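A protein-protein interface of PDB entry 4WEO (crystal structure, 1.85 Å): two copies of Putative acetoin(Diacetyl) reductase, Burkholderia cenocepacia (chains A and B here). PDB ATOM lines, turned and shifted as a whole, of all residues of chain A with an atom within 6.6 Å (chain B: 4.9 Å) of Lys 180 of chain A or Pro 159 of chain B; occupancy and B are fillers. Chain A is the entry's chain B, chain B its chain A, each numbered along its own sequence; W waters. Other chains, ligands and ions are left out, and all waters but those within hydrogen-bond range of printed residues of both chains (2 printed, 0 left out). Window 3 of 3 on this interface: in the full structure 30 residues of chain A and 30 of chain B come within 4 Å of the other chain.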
ATOM      1  N   THR A 175      23.284  20.189  13.108  1.00  0.00           N
ATOM      2  CA  THR A 175      23.684  21.406  12.410  1.00  0.00           C
ATOM      3  C   THR A 175      22.510  22.401  12.380  1.00  0.00           C
ATOM      4  O   THR A 175      22.659  23.578  12.730  1.00  0.00           O
ATOM      5  CB  THR A 175      24.150  21.087  10.945  1.00  0.00           C
ATOM      6  OG1 THR A 175      25.294  20.220  10.965  1.00  0.00           O
ATOM      7  CG2 THR A 175      24.500  22.371  10.173  1.00  0.00           C
ATOM      8  N   ASN A 176      21.341  21.923  11.956  1.00  0.00           N
ATOM      9  CA  ASN A 176      20.180  22.801  11.822  1.00  0.00           C
ATOM     10  C   ASN A 176      19.755  23.335  13.199  1.00  0.00           C
ATOM     11  O   ASN A 176      19.446  24.516  13.362  1.00  0.00           O
ATOM     12  CB  ASN A 176      19.032  22.050  11.139  1.00  0.00           C
ATOM     13  CG  ASN A 176      17.850  22.951  10.806  1.00  0.00           C
ATOM     14  OD1 ASN A 176      16.777  22.804  11.374  1.00  0.00           O
ATOM     15  ND2 ASN A 176      18.055  23.897   9.889  1.00  0.00           N
ATOM     16  N   ALA A 177      19.765  22.461  14.195  1.00  0.00           N
ATOM     17  CA  ALA A 177      19.352  22.853  15.523  1.00  0.00           C
ATOM     18  C   ALA A 177      20.312  23.889  16.110  1.00  0.00           C
ATOM     19  O   ALA A 177      19.884  24.918  16.634  1.00  0.00           O
ATOM     20  CB  ALA A 177      19.254  21.628  16.417  1.00  0.00           C
ATOM     21  N   LEU A 178      21.609  23.628  15.991  1.00  0.00           N
ATOM     22  CA  LEU A 178      22.605  24.544  16.541  1.00  0.00           C
ATOM     23  C   LEU A 178      22.576  25.884  15.805  1.00  0.00           C
ATOM     24  O   LEU A 178      22.745  26.930  16.411  1.00  0.00           O
ATOM     25  CB  LEU A 178      24.004  23.921  16.451  1.00  0.00           C
ATOM     26  CG  LEU A 178      25.135  24.809  16.984  1.00  0.00           C
ATOM     27  CD1 LEU A 178      24.886  25.166  18.457  1.00  0.00           C
ATOM     28  CD2 LEU A 178      26.469  24.104  16.819  1.00  0.00           C
ATOM     29  N   ALA A 179      22.349  25.849  14.495  1.00  0.00           N
ATOM     30  CA  ALA A 179      22.211  27.092  13.727  1.00  0.00           C
ATOM     31  C   ALA A 179      21.140  27.992  14.348  1.00  0.00           C
ATOM     32  O   ALA A 179      21.330  29.202  14.487  1.00  0.00           O
ATOM     33  CB  ALA A 179      21.870  26.790  12.285  1.00  0.00           C
ATOM     34  N   LYS A 180      20.028  27.387  14.754  1.00  0.00           N
ATOM     35  CA  LYS A 180      18.926  28.136  15.362  1.00  0.00           C
ATOM     36  C   LYS A 180      19.278  28.694  16.742  1.00  0.00           C
ATOM     37  O   LYS A 180      18.831  29.780  17.102  1.00  0.00           O
ATOM     38  CB  LYS A 180      17.671  27.250  15.434  1.00  0.00           C
ATOM     39  CG  LYS A 180      17.089  26.975  14.060  1.00  0.00           C
ATOM     40  CD  LYS A 180      15.985  25.921  14.071  1.00  0.00           C
ATOM     41  CE  LYS A 180      15.563  25.570  12.641  1.00  0.00           C
ATOM     42  NZ  LYS A 180      14.556  24.459  12.603  1.00  0.00           N
ATOM     43  N   GLU A 181      20.087  27.969  17.510  1.00  0.00           N
ATOM     44  CA  GLU A 181      20.532  28.467  18.810  1.00  0.00           C
ATOM     45  C   GLU A 181      21.401  29.712  18.686  1.00  0.00           C
ATOM     46  O   GLU A 181      21.353  30.606  19.543  1.00  0.00           O
ATOM     47  CB  GLU A 181      21.303  27.381  19.574  1.00  0.00           C
ATOM     48  CG  GLU A 181      20.489  26.125  19.838  1.00  0.00           C
ATOM     49  CD  GLU A 181      21.140  25.169  20.833  1.00  0.00           C
ATOM     50  OE1 GLU A 181      22.228  25.484  21.383  1.00  0.00           O
ATOM     51  OE2 GLU A 181      20.547  24.094  21.063  1.00  0.00           O
ATOM     52  N   LEU A 182      22.200  29.748  17.621  1.00  0.00           N
ATOM     53  CA  LEU A 182      23.212  30.784  17.412  1.00  0.00           C
ATOM     54  C   LEU A 182      22.827  31.858  16.397  1.00  0.00           C
ATOM     55  O   LEU A 182      23.632  32.743  16.108  1.00  0.00           O
ATOM     56  CB  LEU A 182      24.522  30.136  16.951  1.00  0.00           C
ATOM     57  CG  LEU A 182      25.094  29.099  17.917  1.00  0.00           C
ATOM     58  CD1 LEU A 182      26.363  28.474  17.344  1.00  0.00           C
ATOM     59  CD2 LEU A 182      25.389  29.777  19.233  1.00  0.00           C
ATOM     60  N   ALA A 183      21.592  31.820  15.906  1.00  0.00           N
ATOM     61  CA  ALA A 183      21.204  32.659  14.767  1.00  0.00           C
ATOM     62  C   ALA A 183      21.293  34.152  15.042  1.00  0.00           C
ATOM     63  O   ALA A 183      21.497  34.938  14.115  1.00  0.00           O
ATOM     64  CB  ALA A 183      19.800  32.311  14.316  1.00  0.00           C
ATOM     65  N   ARG A 184      21.152  34.545  16.310  1.00  0.00           N
ATOM     66  CA  ARG A 184      21.223  35.957  16.666  1.00  0.00           C
ATOM     67  C   ARG A 184      22.559  36.285  17.316  1.00  0.00           C
ATOM     68  O   ARG A 184      22.739  37.366  17.866  1.00  0.00           O
ATOM     69  CB  ARG A 184      20.097  36.324  17.633  1.00  0.00           C
ATOM     70  CG  ARG A 184      18.705  36.101  17.088  1.00  0.00           C
ATOM     71  CD  ARG A 184      18.322  37.149  16.086  1.00  0.00           C
ATOM     72  NE  ARG A 184      16.872  37.226  15.935  1.00  0.00           N
ATOM     73  CZ  ARG A 184      16.164  38.343  16.084  1.00  0.00           C
ATOM     74  NH1 ARG A 184      16.772  39.486  16.374  1.00  0.00           N
ATOM     75  NH2 ARG A 184      14.847  38.318  15.927  1.00  0.00           N
ATOM     76  N   VAL A 189      25.955  28.243  11.140  1.00  0.00           N
ATOM     77  CA  VAL A 189      26.227  26.818  11.275  1.00  0.00           C
ATOM     78  C   VAL A 189      25.638  26.114  10.051  1.00  0.00           C
ATOM     79  O   VAL A 189      24.432  26.199   9.796  1.00  0.00           O
ATOM     80  CB  VAL A 189      25.625  26.237  12.593  1.00  0.00           C
ATOM     81  CG1 VAL A 189      26.084  24.795  12.812  1.00  0.00           C
ATOM     82  CG2 VAL A 189      25.979  27.113  13.789  1.00  0.00           C
ATOM     83  N   THR A 253      22.525  30.119   6.928  1.00  0.00           N
ATOM     84  CA  THR A 253      22.762  29.329   8.134  1.00  0.00           C
ATOM     85  C   THR A 253      21.739  28.209   8.204  1.00  0.00           C
ATOM     86  O   THR A 253      20.638  28.330   7.663  1.00  0.00           O
ATOM     87  CB  THR A 253      22.722  30.194   9.430  1.00  0.00           C
ATOM     88  OG1 THR A 253      23.348  29.479  10.500  1.00  0.00           O
ATOM     89  CG2 THR A 253      21.290  30.563   9.845  1.00  0.00           C
ATOM     90  N   GLY A 254      22.124  27.112   8.848  1.00  0.00           N
ATOM     91  CA  GLY A 254      21.244  25.981   9.034  1.00  0.00           C
ATOM     92  C   GLY A 254      21.152  25.037   7.866  1.00  0.00           C
ATOM     93  O   GLY A 254      20.430  24.042   7.952  1.00  0.00           O
ATOM     94  N   GLU B 156      13.189  18.469  11.620  1.00  0.00           N
ATOM     95  CA  GLU B 156      13.635  19.848  11.817  1.00  0.00           C
ATOM     96  C   GLU B 156      14.541  19.879  13.045  1.00  0.00           C
ATOM     97  O   GLU B 156      14.249  19.232  14.063  1.00  0.00           O
ATOM     98  CB  GLU B 156      12.451  20.809  12.023  1.00  0.00           C
ATOM     99  CG  GLU B 156      11.277  20.651  11.052  1.00  0.00           C
ATOM    100  CD  GLU B 156      11.574  21.182   9.658  1.00  0.00           C
ATOM    101  OE1 GLU B 156      12.600  21.882   9.484  1.00  0.00           O
ATOM    102  OE2 GLU B 156      10.778  20.892   8.733  1.00  0.00           O
ATOM    103  N   GLY B 157      15.640  20.621  12.971  1.00  0.00           N
ATOM    104  CA  GLY B 157      16.462  20.789  14.158  1.00  0.00           C
ATOM    105  C   GLY B 157      15.767  21.714  15.137  1.00  0.00           C
ATOM    106  O   GLY B 157      15.350  22.816  14.768  1.00  0.00           O
ATOM    107  N   PHE B 158      15.638  21.272  16.386  1.00  0.00           N
ATOM    108  CA  PHE B 158      15.052  22.099  17.440  1.00  0.00           C
ATOM    109  C   PHE B 158      16.128  22.712  18.335  1.00  0.00           C
ATOM    110  O   PHE B 158      16.940  21.990  18.904  1.00  0.00           O
ATOM    111  CB  PHE B 158      14.090  21.270  18.306  1.00  0.00           C
ATOM    112  CG  PHE B 158      12.727  21.097  17.702  1.00  0.00           C
ATOM    113  CD1 PHE B 158      12.541  20.282  16.596  1.00  0.00           C
ATOM    114  CD2 PHE B 158      11.630  21.760  18.235  1.00  0.00           C
ATOM    115  CE1 PHE B 158      11.273  20.123  16.027  1.00  0.00           C
ATOM    116  CE2 PHE B 158      10.364  21.612  17.672  1.00  0.00           C
ATOM    117  CZ  PHE B 158      10.193  20.785  16.572  1.00  0.00           C
ATOM    118  N   PRO B 159      16.121  24.045  18.485  1.00  0.00           N
ATOM    119  CA  PRO B 159      17.068  24.689  19.409  1.00  0.00           C
ATOM    120  C   PRO B 159      16.853  24.225  20.859  1.00  0.00           C
ATOM    121  O   PRO B 159      15.703  23.989  21.251  1.00  0.00           O
ATOM    122  CB  PRO B 159      16.775  26.187  19.242  1.00  0.00           C
ATOM    123  CG  PRO B 159      15.402  26.262  18.596  1.00  0.00           C
ATOM    124  CD  PRO B 159      15.221  25.003  17.816  1.00  0.00           C
ATOM    125  N   ASN B 160      17.951  24.068  21.608  1.00  0.00           N
ATOM    126  CA  ASN B 160      17.955  23.516  22.976  1.00  0.00           C
ATOM    127  C   ASN B 160      17.581  22.029  23.011  1.00  0.00           C
ATOM    128  O   ASN B 160      17.420  21.426  24.086  1.00  0.00           O
ATOM    129  CB  ASN B 160      17.026  24.322  23.875  1.00  0.00           C
ATOM    130  CG  ASN B 160      17.359  25.791  23.851  1.00  0.00           C
ATOM    131  OD1 ASN B 160      18.527  26.167  23.879  1.00  0.00           O
ATOM    132  ND2 ASN B 160      16.340  26.629  23.731  1.00  0.00           N
ATOM    133  N   LEU B 161      17.464  21.457  21.818  1.00  0.00           N
ATOM    134  CA  LEU B 161      17.227  20.035  21.614  1.00  0.00           C
ATOM    135  C   LEU B 161      18.111  19.460  20.526  1.00  0.00           C
ATOM    136  O   LEU B 161      17.687  18.566  19.811  1.00  0.00           O
ATOM    137  CB  LEU B 161      15.767  19.786  21.241  1.00  0.00           C
ATOM    138  CG  LEU B 161      14.805  19.952  22.410  1.00  0.00           C
ATOM    139  CD1 LEU B 161      13.408  19.874  21.895  1.00  0.00           C
ATOM    140  CD2 LEU B 161      15.031  18.852  23.374  1.00  0.00           C
HETATM  141  O   HOH W   1      20.791  21.703  22.143  1.00  0.00           O
HETATM  142  O   HOH W   2      13.872  23.968  10.122  1.00  0.00           O
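The side-chain amide oxygen of Asn 176 of chain A is in hydrogen-bond range of the backbone NH of Gly 157 of chain B (2.9 Å).
The side-chain amino group (NZ) of Lys 180 of chain A is in hydrogen-bond range of the backbone carbonyl oxygen (O) of Gly 157 of chain B, at 2.8 Å.
The backbone NH (N) of Asn 160 of chain B is in hydrogen-bond range of the side-chain carboxylate (OE2) of Glu 181 of chain A, at 2.7 Å.
ND2 of Asn 176 of chain A is in hydrogen-bond range of O of Gly 254 of chain A (3.1 Å).
The side-chain amide oxygen (OD1) of Asn 176 of chain A is in hydrogen-bond range of the side-chain amino group (NZ) of Lys 180 of chain A, 3.0 Å away.
Ala 177 of chain A touches Gly 157 of chain B (CB to CA, 3.7 Å).
O of Phe 158 of chain B touches CB of Ala 177 of chain A, at 3.4 Å.
CA of Pro 159 of chain B touches O of Ala 177 of chain A, at 3.96 Å.
Lys 180 of chain A touches Pro 159 of chain B.
C of Pro 159 of chain B touches OE2 of Glu 181 of chain A, at 3.7 Å.
Lys 180 of chain A touches just these residues of chain B: Gly 157 (2.8 Å) and Pro 159 (3.9 Å).
Pro 159 of chain B touches three residues of chain A.
Of the printed residues of chain B, Ala 177 of chain A touches Gly 157, Phe 158 and Pro 159.
Printed residues of chain A within 4 Å of Asn 160 of chain B: Glu 181.
Printed residues of chain A within 4 Å of Phe 158 of chain B: Ala 177.
Ala 179 of chain A touches none of the printed residues of chain B.
Thr 253 of chain A touches none of the printed residues of chain B.
The nearest residue of chain A that does not touch Pro 159 of chain B is Leu 178 of chain A (5.8 Å).
The nearest printed residue of chain B that does not touch Asn 176 of chain A is Glu 156 of chain B (4.04 Å).
Of the 13 printed residues of chain A, 4 touch a printed residue of chain B.
No position is printed for both chains.
Of the 8 pairs that touch across the chains among the printed residues, none has its exchanged pair printed and touching as well.
Water W2 lies within hydrogen-bond range of the side-chain carboxylate (OE1) of Glu 156 of chain B (2.5 Å), the side-chain amino group (NZ) of Lys 180 of chain A (2.6 Å) and the side-chain amide oxygen (OD1) of Asn 176 of chain A (3.4 Å).
Water W1 bridges OE2 of Glu 181 of chain A (2.6 Å) and N of Leu 161 of chain B (3.4 Å).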
